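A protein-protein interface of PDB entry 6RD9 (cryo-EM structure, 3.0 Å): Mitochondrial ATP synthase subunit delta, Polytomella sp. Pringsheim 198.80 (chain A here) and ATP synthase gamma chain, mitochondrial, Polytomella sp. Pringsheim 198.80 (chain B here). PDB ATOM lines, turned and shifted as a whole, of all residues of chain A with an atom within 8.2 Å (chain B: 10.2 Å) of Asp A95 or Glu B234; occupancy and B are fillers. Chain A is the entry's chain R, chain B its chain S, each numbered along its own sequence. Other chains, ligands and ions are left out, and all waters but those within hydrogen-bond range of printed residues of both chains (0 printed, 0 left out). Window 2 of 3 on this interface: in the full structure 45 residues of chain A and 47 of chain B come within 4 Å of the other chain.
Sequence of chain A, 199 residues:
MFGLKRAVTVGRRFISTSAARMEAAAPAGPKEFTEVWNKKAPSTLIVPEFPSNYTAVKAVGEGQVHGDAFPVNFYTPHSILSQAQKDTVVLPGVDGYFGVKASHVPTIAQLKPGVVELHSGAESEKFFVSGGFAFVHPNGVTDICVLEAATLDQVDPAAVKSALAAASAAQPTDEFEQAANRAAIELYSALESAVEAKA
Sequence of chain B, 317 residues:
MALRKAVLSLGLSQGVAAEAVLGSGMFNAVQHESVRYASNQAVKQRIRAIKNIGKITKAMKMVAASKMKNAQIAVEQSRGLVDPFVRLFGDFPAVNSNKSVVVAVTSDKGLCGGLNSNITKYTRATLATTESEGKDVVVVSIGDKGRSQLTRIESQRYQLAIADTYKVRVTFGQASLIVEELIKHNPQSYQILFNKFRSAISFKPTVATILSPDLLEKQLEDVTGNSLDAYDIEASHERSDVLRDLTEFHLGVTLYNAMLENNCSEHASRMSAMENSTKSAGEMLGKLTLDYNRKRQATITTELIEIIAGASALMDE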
ATOM      1  N   LEU A  91      25.613  14.380  -5.078  1.00  0.00           N
ATOM      2  CA  LEU A  91      26.332  14.086  -6.296  1.00  0.00           C
ATOM      3  C   LEU A  91      27.702  14.722  -6.249  1.00  0.00           C
ATOM      4  O   LEU A  91      27.818  15.873  -5.821  1.00  0.00           O
ATOM      5  CB  LEU A  91      25.557  14.613  -7.488  1.00  0.00           C
ATOM      6  CG  LEU A  91      24.339  13.775  -7.807  1.00  0.00           C
ATOM      7  CD1 LEU A  91      23.491  14.461  -8.825  1.00  0.00           C
ATOM      8  CD2 LEU A  91      24.817  12.461  -8.329  1.00  0.00           C
ATOM      9  N   PRO A  92      28.744  14.038  -6.658  1.00  0.00           N
ATOM     10  CA  PRO A  92      30.100  14.612  -6.584  1.00  0.00           C
ATOM     11  C   PRO A  92      30.511  15.397  -7.827  1.00  0.00           C
ATOM     12  O   PRO A  92      31.351  14.961  -8.611  1.00  0.00           O
ATOM     13  CB  PRO A  92      30.958  13.365  -6.389  1.00  0.00           C
ATOM     14  CG  PRO A  92      30.221  12.302  -7.123  1.00  0.00           C
ATOM     15  CD  PRO A  92      28.763  12.637  -7.095  1.00  0.00           C
ATOM     16  N   GLY A  93      29.941  16.594  -8.000  1.00  0.00           N
ATOM     17  CA  GLY A  93      30.220  17.390  -9.181  1.00  0.00           C
ATOM     18  C   GLY A  93      31.649  17.894  -9.225  1.00  0.00           C
ATOM     19  O   GLY A  93      32.392  17.811  -8.254  1.00  0.00           O
ATOM     20  N   VAL A  94      32.055  18.407 -10.388  1.00  0.00           N
ATOM     21  CA  VAL A  94      33.440  18.839 -10.525  1.00  0.00           C
ATOM     22  C   VAL A  94      33.701  20.155  -9.817  1.00  0.00           C
ATOM     23  O   VAL A  94      34.851  20.449  -9.475  1.00  0.00           O
ATOM     24  CB  VAL A  94      33.875  18.950 -11.995  1.00  0.00           C
ATOM     25  CG1 VAL A  94      33.962  17.596 -12.622  1.00  0.00           C
ATOM     26  CG2 VAL A  94      32.926  19.806 -12.750  1.00  0.00           C
ATOM     27  N   ASP A  95      32.672  20.966  -9.587  1.00  0.00           N
ATOM     28  CA  ASP A  95      32.847  22.136  -8.741  1.00  0.00           C
ATOM     29  C   ASP A  95      32.910  21.712  -7.285  1.00  0.00           C
ATOM     30  O   ASP A  95      33.797  22.131  -6.535  1.00  0.00           O
ATOM     31  CB  ASP A  95      31.710  23.123  -8.976  1.00  0.00           C
ATOM     32  CG  ASP A  95      31.650  23.606 -10.408  1.00  0.00           C
ATOM     33  OD1 ASP A  95      30.615  24.179 -10.795  1.00  0.00           O
ATOM     34  OD2 ASP A  95      32.634  23.416 -11.152  1.00  0.00           O
ATOM     35  N   GLY A  96      31.972  20.872  -6.876  1.00  0.00           N
ATOM     36  CA  GLY A  96      32.009  20.256  -5.567  1.00  0.00           C
ATOM     37  C   GLY A  96      30.776  19.410  -5.386  1.00  0.00           C
ATOM     38  O   GLY A  96      29.925  19.322  -6.271  1.00  0.00           O
ATOM     39  N   TYR A  97      30.688  18.792  -4.213  1.00  0.00           N
ATOM     40  CA  TYR A  97      29.551  17.948  -3.881  1.00  0.00           C
ATOM     41  C   TYR A  97      28.301  18.797  -3.773  1.00  0.00           C
ATOM     42  O   TYR A  97      28.234  19.699  -2.940  1.00  0.00           O
ATOM     43  CB  TYR A  97      29.790  17.222  -2.563  1.00  0.00           C
ATOM     44  CG  TYR A  97      30.688  16.023  -2.640  1.00  0.00           C
ATOM     45  CD1 TYR A  97      32.060  16.171  -2.722  1.00  0.00           C
ATOM     46  CD2 TYR A  97      30.168  14.744  -2.615  1.00  0.00           C
ATOM     47  CE1 TYR A  97      32.889  15.088  -2.785  1.00  0.00           C
ATOM     48  CE2 TYR A  97      30.992  13.651  -2.679  1.00  0.00           C
ATOM     49  CZ  TYR A  97      32.352  13.831  -2.764  1.00  0.00           C
ATOM     50  OH  TYR A  97      33.189  12.746  -2.827  1.00  0.00           O
ATOM     51  N   PHE A  98      27.321  18.533  -4.612  1.00  0.00           N
ATOM     52  CA  PHE A  98      26.038  19.192  -4.476  1.00  0.00           C
ATOM     53  C   PHE A  98      24.961  18.168  -4.171  1.00  0.00           C
ATOM     54  O   PHE A  98      25.167  16.962  -4.283  1.00  0.00           O
ATOM     55  CB  PHE A  98      25.696  20.016  -5.719  1.00  0.00           C
ATOM     56  CG  PHE A  98      25.495  19.219  -6.968  1.00  0.00           C
ATOM     57  CD1 PHE A  98      26.572  18.797  -7.721  1.00  0.00           C
ATOM     58  CD2 PHE A  98      24.223  18.965  -7.436  1.00  0.00           C
ATOM     59  CE1 PHE A  98      26.386  18.094  -8.864  1.00  0.00           C
ATOM     60  CE2 PHE A  98      24.035  18.266  -8.592  1.00  0.00           C
ATOM     61  CZ  PHE A  98      25.117  17.829  -9.298  1.00  0.00           C
ATOM     62  N   PRO A 106      17.007  22.251 -13.665  1.00  0.00           N
ATOM     63  CA  PRO A 106      17.621  21.386 -14.677  1.00  0.00           C
ATOM     64  C   PRO A 106      19.129  21.567 -14.757  1.00  0.00           C
ATOM     65  O   PRO A 106      19.643  22.686 -14.758  1.00  0.00           O
ATOM     66  CB  PRO A 106      16.932  21.823 -15.967  1.00  0.00           C
ATOM     67  CG  PRO A 106      15.597  22.246 -15.524  1.00  0.00           C
ATOM     68  CD  PRO A 106      15.746  22.834 -14.151  1.00  0.00           C
ATOM     69  N   THR A 107      19.833  20.441 -14.832  1.00  0.00           N
ATOM     70  CA  THR A 107      21.260  20.376 -14.560  1.00  0.00           C
ATOM     71  C   THR A 107      21.879  19.324 -15.463  1.00  0.00           C
ATOM     72  O   THR A 107      21.308  18.248 -15.619  1.00  0.00           O
ATOM     73  CB  THR A 107      21.482  20.027 -13.083  1.00  0.00           C
ATOM     74  OG1 THR A 107      21.027  21.108 -12.263  1.00  0.00           O
ATOM     75  CG2 THR A 107      22.928  19.761 -12.771  1.00  0.00           C
ATOM     76  N   ILE A 108      23.004  19.645 -16.094  1.00  0.00           N
ATOM     77  CA  ILE A 108      23.888  18.657 -16.702  1.00  0.00           C
ATOM     78  C   ILE A 108      25.208  18.760 -15.964  1.00  0.00           C
ATOM     79  O   ILE A 108      25.964  19.712 -16.169  1.00  0.00           O
ATOM     80  CB  ILE A 108      24.083  18.883 -18.200  1.00  0.00           C
ATOM     81  CG1 ILE A 108      22.776  18.685 -18.934  1.00  0.00           C
ATOM     82  CG2 ILE A 108      25.099  17.927 -18.745  1.00  0.00           C
ATOM     83  CD1 ILE A 108      22.857  19.073 -20.369  1.00  0.00           C
ATOM     84  N   ALA A 109      25.485  17.805 -15.093  1.00  0.00           N
ATOM     85  CA  ALA A 109      26.598  17.923 -14.171  1.00  0.00           C
ATOM     86  C   ALA A 109      27.614  16.843 -14.459  1.00  0.00           C
ATOM     87  O   ALA A 109      27.311  15.660 -14.327  1.00  0.00           O
ATOM     88  CB  ALA A 109      26.120  17.820 -12.731  1.00  0.00           C
ATOM     89  N   GLN A 110      28.808  17.241 -14.855  1.00  0.00           N
ATOM     90  CA  GLN A 110      29.902  16.297 -14.957  1.00  0.00           C
ATOM     91  C   GLN A 110      30.435  16.016 -13.569  1.00  0.00           C
ATOM     92  O   GLN A 110      30.728  16.945 -12.819  1.00  0.00           O
ATOM     93  CB  GLN A 110      31.006  16.840 -15.849  1.00  0.00           C
ATOM     94  CG  GLN A 110      32.232  15.966 -15.869  1.00  0.00           C
ATOM     95  CD  GLN A 110      33.276  16.449 -16.839  1.00  0.00           C
ATOM     96  OE1 GLN A 110      32.980  17.207 -17.762  1.00  0.00           O
ATOM     97  NE2 GLN A 110      34.511  16.018 -16.638  1.00  0.00           N
ATOM     98  N   LEU A 111      30.549  14.746 -13.215  1.00  0.00           N
ATOM     99  CA  LEU A 111      30.935  14.368 -11.869  1.00  0.00           C
ATOM    100  C   LEU A 111      32.396  13.951 -11.806  1.00  0.00           C
ATOM    101  O   LEU A 111      32.920  13.326 -12.727  1.00  0.00           O
ATOM    102  CB  LEU A 111      30.051  13.242 -11.350  1.00  0.00           C
ATOM    103  CG  LEU A 111      28.550  13.474 -11.449  1.00  0.00           C
ATOM    104  CD1 LEU A 111      27.829  12.272 -10.923  1.00  0.00           C
ATOM    105  CD2 LEU A 111      28.140  14.691 -10.700  1.00  0.00           C
ATOM    106  N   LYS A 112      33.048  14.323 -10.715  1.00  0.00           N
ATOM    107  CA  LYS A 112      34.375  13.845 -10.371  1.00  0.00           C
ATOM    108  C   LYS A 112      34.288  12.422  -9.856  1.00  0.00           C
ATOM    109  O   LYS A 112      33.201  11.920  -9.577  1.00  0.00           O
ATOM    110  CB  LYS A 112      34.987  14.747  -9.303  1.00  0.00           C
ATOM    111  CG  LYS A 112      35.764  15.918  -9.820  1.00  0.00           C
ATOM    112  CD  LYS A 112      35.999  16.916  -8.709  1.00  0.00           C
ATOM    113  CE  LYS A 112      36.909  16.393  -7.633  1.00  0.00           C
ATOM    114  NZ  LYS A 112      37.158  17.461  -6.631  1.00  0.00           N
ATOM    115  N   PHE A 133      28.590  11.614 -15.959  1.00  0.00           N
ATOM    116  CA  PHE A 133      27.689  12.736 -15.817  1.00  0.00           C
ATOM    117  C   PHE A 133      26.465  12.373 -14.995  1.00  0.00           C
ATOM    118  O   PHE A 133      26.214  11.217 -14.675  1.00  0.00           O
ATOM    119  CB  PHE A 133      27.262  13.229 -17.188  1.00  0.00           C
ATOM    120  CG  PHE A 133      28.404  13.532 -18.087  1.00  0.00           C
ATOM    121  CD1 PHE A 133      28.995  14.770 -18.061  1.00  0.00           C
ATOM    122  CD2 PHE A 133      28.890  12.584 -18.960  1.00  0.00           C
ATOM    123  CE1 PHE A 133      30.057  15.051 -18.871  1.00  0.00           C
ATOM    124  CE2 PHE A 133      29.930  12.867 -19.781  1.00  0.00           C
ATOM    125  CZ  PHE A 133      30.521  14.101 -19.734  1.00  0.00           C
ATOM    126  N   ALA A 134      25.706  13.403 -14.640  1.00  0.00           N
ATOM    127  CA  ALA A 134      24.442  13.248 -13.937  1.00  0.00           C
ATOM    128  C   ALA A 134      23.524  14.352 -14.414  1.00  0.00           C
ATOM    129  O   ALA A 134      23.855  15.526 -14.265  1.00  0.00           O
ATOM    130  CB  ALA A 134      24.627  13.337 -12.431  1.00  0.00           C
ATOM    131  N   LEU B 228      18.158  22.729 -25.011  1.00  0.00           N
ATOM    132  CA  LEU B 228      19.282  22.387 -24.161  1.00  0.00           C
ATOM    133  C   LEU B 228      19.594  23.479 -23.150  1.00  0.00           C
ATOM    134  O   LEU B 228      20.191  23.192 -22.108  1.00  0.00           O
ATOM    135  CB  LEU B 228      20.497  22.110 -25.052  1.00  0.00           C
ATOM    136  CG  LEU B 228      21.912  21.879 -24.551  1.00  0.00           C
ATOM    137  CD1 LEU B 228      22.080  20.440 -24.151  1.00  0.00           C
ATOM    138  CD2 LEU B 228      22.870  22.248 -25.664  1.00  0.00           C
ATOM    139  N   ALA B 230      17.713  24.834 -21.063  1.00  0.00           N
ATOM    140  CA  ALA B 230      17.033  24.696 -19.786  1.00  0.00           C
ATOM    141  C   ALA B 230      17.983  24.215 -18.701  1.00  0.00           C
ATOM    142  O   ALA B 230      17.792  24.535 -17.526  1.00  0.00           O
ATOM    143  CB  ALA B 230      15.857  23.736 -19.925  1.00  0.00           C
ATOM    144  N   TYR B 231      19.023  23.480 -19.079  1.00  0.00           N
ATOM    145  CA  TYR B 231      19.898  22.816 -18.129  1.00  0.00           C
ATOM    146  C   TYR B 231      21.048  23.714 -17.729  1.00  0.00           C
ATOM    147  O   TYR B 231      21.671  24.361 -18.571  1.00  0.00           O
ATOM    148  CB  TYR B 231      20.462  21.528 -18.721  1.00  0.00           C
ATOM    149  CG  TYR B 231      19.427  20.526 -19.138  1.00  0.00           C
ATOM    150  CD1 TYR B 231      18.952  19.588 -18.243  1.00  0.00           C
ATOM    151  CD2 TYR B 231      18.931  20.517 -20.424  1.00  0.00           C
ATOM    152  CE1 TYR B 231      18.015  18.678 -18.617  1.00  0.00           C
ATOM    153  CE2 TYR B 231      17.993  19.616 -20.801  1.00  0.00           C
ATOM    154  CZ  TYR B 231      17.539  18.701 -19.898  1.00  0.00           C
ATOM    155  OH  TYR B 231      16.595  17.793 -20.292  1.00  0.00           O
ATOM    156  N   ASP B 232      21.359  23.705 -16.446  1.00  0.00           N
ATOM    157  CA  ASP B 232      22.469  24.476 -15.923  1.00  0.00           C
ATOM    158  C   ASP B 232      23.712  23.603 -15.984  1.00  0.00           C
ATOM    159  O   ASP B 232      23.791  22.587 -15.290  1.00  0.00           O
ATOM    160  CB  ASP B 232      22.160  24.925 -14.495  1.00  0.00           C
ATOM    161  CG  ASP B 232      23.041  26.060 -14.027  1.00  0.00           C
ATOM    162  OD1 ASP B 232      23.900  26.523 -14.805  1.00  0.00           O
ATOM    163  OD2 ASP B 232      22.871  26.492 -12.871  1.00  0.00           O
ATOM    164  N   ILE B 233      24.677  23.992 -16.810  1.00  0.00           N
ATOM    165  CA  ILE B 233      25.850  23.157 -17.044  1.00  0.00           C
ATOM    166  C   ILE B 233      26.793  23.277 -15.859  1.00  0.00           C
ATOM    167  O   ILE B 233      27.195  24.378 -15.474  1.00  0.00           O
ATOM    168  CB  ILE B 233      26.558  23.551 -18.342  1.00  0.00           C
ATOM    169  CG1 ILE B 233      25.565  23.635 -19.489  1.00  0.00           C
ATOM    170  CG2 ILE B 233      27.636  22.555 -18.667  1.00  0.00           C
ATOM    171  CD1 ILE B 233      24.869  22.348 -19.780  1.00  0.00           C
ATOM    172  N   GLU B 234      27.160  22.141 -15.280  1.00  0.00           N
ATOM    173  CA  GLU B 234      28.094  22.099 -14.169  1.00  0.00           C
ATOM    174  C   GLU B 234      29.427  21.496 -14.593  1.00  0.00           C
ATOM    175  O   GLU B 234      30.010  20.700 -13.870  1.00  0.00           O
ATOM    176  CB  GLU B 234      27.454  21.328 -13.011  1.00  0.00           C
ATOM    177  CG  GLU B 234      27.955  21.615 -11.596  1.00  0.00           C
ATOM    178  CD  GLU B 234      28.909  20.563 -11.080  1.00  0.00           C
ATOM    179  OE1 GLU B 234      28.798  19.400 -11.497  1.00  0.00           O
ATOM    180  OE2 GLU B 234      29.778  20.892 -10.260  1.00  0.00           O
ATOM    181  N   ALA B 235      29.907  21.828 -15.778  1.00  0.00           N
ATOM    182  CA  ALA B 235      31.142  21.211 -16.219  1.00  0.00           C
ATOM    183  C   ALA B 235      32.341  22.059 -15.838  1.00  0.00           C
ATOM    184  O   ALA B 235      32.218  23.153 -15.288  1.00  0.00           O
ATOM    185  CB  ALA B 235      31.130  20.992 -17.723  1.00  0.00           C
ATOM    186  N   SER B 236      33.521  21.535 -16.144  1.00  0.00           N
ATOM    187  CA  SER B 236      34.738  22.320 -15.990  1.00  0.00           C
ATOM    188  C   SER B 236      34.815  23.417 -17.043  1.00  0.00           C
ATOM    189  O   SER B 236      35.004  24.592 -16.721  1.00  0.00           O
ATOM    190  CB  SER B 236      35.958  21.411 -16.077  1.00  0.00           C
ATOM    191  OG  SER B 236      37.148  22.169 -16.041  1.00  0.00           O
ATOM    192  N   HIS B 237      34.687  23.047 -18.304  1.00  0.00           N
ATOM    193  CA  HIS B 237      34.771  23.936 -19.438  1.00  0.00           C
ATOM    194  C   HIS B 237      33.385  24.175 -20.032  1.00  0.00           C
ATOM    195  O   HIS B 237      32.371  24.019 -19.346  1.00  0.00           O
ATOM    196  CB  HIS B 237      35.783  23.369 -20.409  1.00  0.00           C
ATOM    197  CG  HIS B 237      37.176  23.414 -19.880  1.00  0.00           C
ATOM    198  ND1 HIS B 237      37.624  22.566 -18.892  1.00  0.00           N
ATOM    199  CD2 HIS B 237      38.215  24.226 -20.177  1.00  0.00           C
ATOM    200  CE1 HIS B 237      38.884  22.843 -18.615  1.00  0.00           C
ATOM    201  NE2 HIS B 237      39.268  23.843 -19.383  1.00  0.00           N
ATOM    202  N   GLU B 238      33.350  24.629 -21.280  1.00  0.00           N
ATOM    203  CA  GLU B 238      32.144  25.169 -21.887  1.00  0.00           C
ATOM    204  C   GLU B 238      31.094  24.092 -22.132  1.00  0.00           C
ATOM    205  O   GLU B 238      31.355  22.892 -22.051  1.00  0.00           O
ATOM    206  CB  GLU B 238      32.469  25.845 -23.214  1.00  0.00           C
ATOM    207  CG  GLU B 238      33.680  26.752 -23.190  1.00  0.00           C
ATOM    208  CD  GLU B 238      33.694  27.669 -21.993  1.00  0.00           C
ATOM    209  OE1 GLU B 238      34.674  27.610 -21.224  1.00  0.00           O
ATOM    210  OE2 GLU B 238      32.717  28.425 -21.814  1.00  0.00           O
ATOM    211  N   ARG B 239      29.884  24.557 -22.449  1.00  0.00           N
ATOM    212  CA  ARG B 239      28.805  23.654 -22.821  1.00  0.00           C
ATOM    213  C   ARG B 239      29.107  22.951 -24.132  1.00  0.00           C
ATOM    214  O   ARG B 239      28.806  21.765 -24.295  1.00  0.00           O
ATOM    215  CB  ARG B 239      27.497  24.421 -22.937  1.00  0.00           C
ATOM    216  CG  ARG B 239      26.314  23.538 -23.194  1.00  0.00           C
ATOM    217  CD  ARG B 239      25.059  24.331 -23.287  1.00  0.00           C
ATOM    218  NE  ARG B 239      25.022  25.092 -24.522  1.00  0.00           N
ATOM    219  CZ  ARG B 239      23.922  25.645 -25.008  1.00  0.00           C
ATOM    220  NH1 ARG B 239      22.779  25.516 -24.352  1.00  0.00           N
ATOM    221  NH2 ARG B 239      23.966  26.324 -26.141  1.00  0.00           N
ATOM    222  N   ASP B 241      31.929  22.068 -24.943  1.00  0.00           N
ATOM    223  CA  ASP B 241      33.014  21.174 -24.595  1.00  0.00           C
ATOM    224  C   ASP B 241      32.522  19.981 -23.792  1.00  0.00           C
ATOM    225  O   ASP B 241      33.074  18.884 -23.910  1.00  0.00           O
ATOM    226  CB  ASP B 241      34.045  21.959 -23.803  1.00  0.00           C
ATOM    227  CG  ASP B 241      35.419  21.437 -23.981  1.00  0.00           C
ATOM    228  OD1 ASP B 241      35.641  20.216 -23.877  1.00  0.00           O
ATOM    229  OD2 ASP B 241      36.282  22.278 -24.280  1.00  0.00           O
ATOM    230  N   VAL B 242      31.487  20.175 -22.974  1.00  0.00           N
ATOM    231  CA  VAL B 242      30.928  19.042 -22.255  1.00  0.00           C
ATOM    232  C   VAL B 242      30.097  18.193 -23.201  1.00  0.00           C
ATOM    233  O   VAL B 242      30.068  16.971 -23.062  1.00  0.00           O
ATOM    234  CB  VAL B 242      30.134  19.503 -21.009  1.00  0.00           C
ATOM    235  CG1 VAL B 242      28.841  20.183 -21.349  1.00  0.00           C
ATOM    236  CG2 VAL B 242      29.842  18.366 -20.113  1.00  0.00           C
ATOM    237  N   LEU B 243      29.489  18.799 -24.228  1.00  0.00           N
ATOM    238  CA  LEU B 243      28.741  18.026 -25.213  1.00  0.00           C
ATOM    239  C   LEU B 243      29.662  17.228 -26.111  1.00  0.00           C
ATOM    240  O   LEU B 243      29.246  16.215 -26.674  1.00  0.00           O
ATOM    241  CB  LEU B 243      27.863  18.941 -26.055  1.00  0.00           C
ATOM    242  CG  LEU B 243      26.379  18.964 -25.740  1.00  0.00           C
ATOM    243  CD1 LEU B 243      26.126  19.554 -24.392  1.00  0.00           C
ATOM    244  CD2 LEU B 243      25.676  19.779 -26.786  1.00  0.00           C
ATOM    245  N   ASP B 245      32.234  15.785 -24.719  1.00  0.00           N
ATOM    246  CA  ASP B 245      32.437  14.637 -23.843  1.00  0.00           C
ATOM    247  C   ASP B 245      31.196  13.761 -23.790  1.00  0.00           C
ATOM    248  O   ASP B 245      31.294  12.545 -23.613  1.00  0.00           O
ATOM    249  CB  ASP B 245      32.795  15.100 -22.432  1.00  0.00           C
ATOM    250  CG  ASP B 245      34.146  15.782 -22.355  1.00  0.00           C
ATOM    251  OD1 ASP B 245      35.025  15.486 -23.186  1.00  0.00           O
ATOM    252  OD2 ASP B 245      34.332  16.609 -21.441  1.00  0.00           O
ATOM    253  N   LEU B 246      30.028  14.362 -23.968  1.00  0.00           N
ATOM    254  CA  LEU B 246      28.767  13.716 -23.638  1.00  0.00           C
ATOM    255  C   LEU B 246      28.228  12.887 -24.788  1.00  0.00           C
ATOM    256  O   LEU B 246      27.475  11.940 -24.561  1.00  0.00           O
ATOM    257  CB  LEU B 246      27.753  14.776 -23.225  1.00  0.00           C
ATOM    258  CG  LEU B 246      26.422  14.442 -22.587  1.00  0.00           C
ATOM    259  CD1 LEU B 246      26.653  13.512 -21.487  1.00  0.00           C
ATOM    260  CD2 LEU B 246      25.825  15.696 -22.043  1.00  0.00           C
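The backbone NH (N) of Val A94 is in hydrogen-bond range of the side-chain carboxylate (OE2) of Glu B234 (3.4 Å).
The side-chain carboxylate (OE2) of Glu B234 sits at hydrogen-bond distance from the backbone NH (N) of Asp A95.
The backbone carbonyl oxygen (O) of Pro A106 sits at hydrogen-bond distance from the backbone NH (N) of Asp B232 (2.6 Å).
The backbone carbonyl oxygen (O) of Asp B232 lies within hydrogen-bond range of the backbone NH (N) of Ile A108 (3.1 Å).
The backbone NH of Glu B234 lies within hydrogen-bond range of the backbone carbonyl oxygen of Ile A108.
The side-chain carboxylate (OE1) of Glu B234 sits close to the backbone carbonyl oxygen (O) of Gln A110, at 3.4 Å.
The backbone carbonyl oxygen of Phe A98 lies within hydrogen-bond range of the backbone NH of Leu A91 (2.7 Å).
The backbone carbonyl oxygen (O) of Gln A110 sits at hydrogen-bond distance from the backbone NH (N) of Val A94, at 3.1 Å.
The backbone carbonyl oxygen (O) of Ala A109 lies within hydrogen-bond range of the backbone NH (N) of Ala A134.
The side-chain hydroxyl of Ser B236 sits at hydrogen-bond distance from a ring nitrogen (ND1) of His B237.
Among the printed residues, pairs that only touch across the chains: Gly A93 with Glu B234, Val A94 with Ala B235, Val A94 with Ser B236, Phe A98 with Glu B234, Pro A106 with Ala B230, Pro A106 with Tyr B231, Thr A107 with Tyr B231, Thr A107 with Asp B232, Ile A108 with Tyr B231, Ile A108 with Ile B233, Ala A109 with Glu B234, Gln A110 with Asp B245, Phe A133 with Val B242, Phe A133 with Asp B245 and Phe A133 with Leu B246.
Leu A91 touches none of the printed residues of chain B.
Gly A93 touches just one residue of chain B: Glu B234.
Asp A95 touches one residue of chain B.
Printed residues of chain B within 4 Å of Pro A106: Ala B230 (3.2 Å), Tyr B231 (3.4 Å) and Asp B232 (2.6 Å).
Ala A109 touches just one residue of chain B: Glu B234.
Leu A111 touches none of the printed residues of chain B.
Of the printed residues of chain B, Phe A133 touches Val B242, Asp B245 and Leu B246.
Printed residues of chain A within 4 Å of Ala B235: Val A94.
Of the printed residues of chain A, Val B242 touches Phe A133.
The nearest residue of chain B that does not touch Asp A95 is Ala B235 (4.2 Å).
The nearest residue of chain A that does not touch Glu B234 is Gly A96 (4.03 Å).
Printed residues of chain B that touch a printed residue of chain A: Ala B230, Tyr B231, Asp B232, Ile B233, Glu B234, Ala B235, Ser B236, Val B242, Asp B245 and Leu B246.
Hydrophobic or aromatic side chains of chain A within 4 Å of the printed part of chain B: Val A94, Phe A98, Pro A106, Ile A108, Ala A109 and Phe A133.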
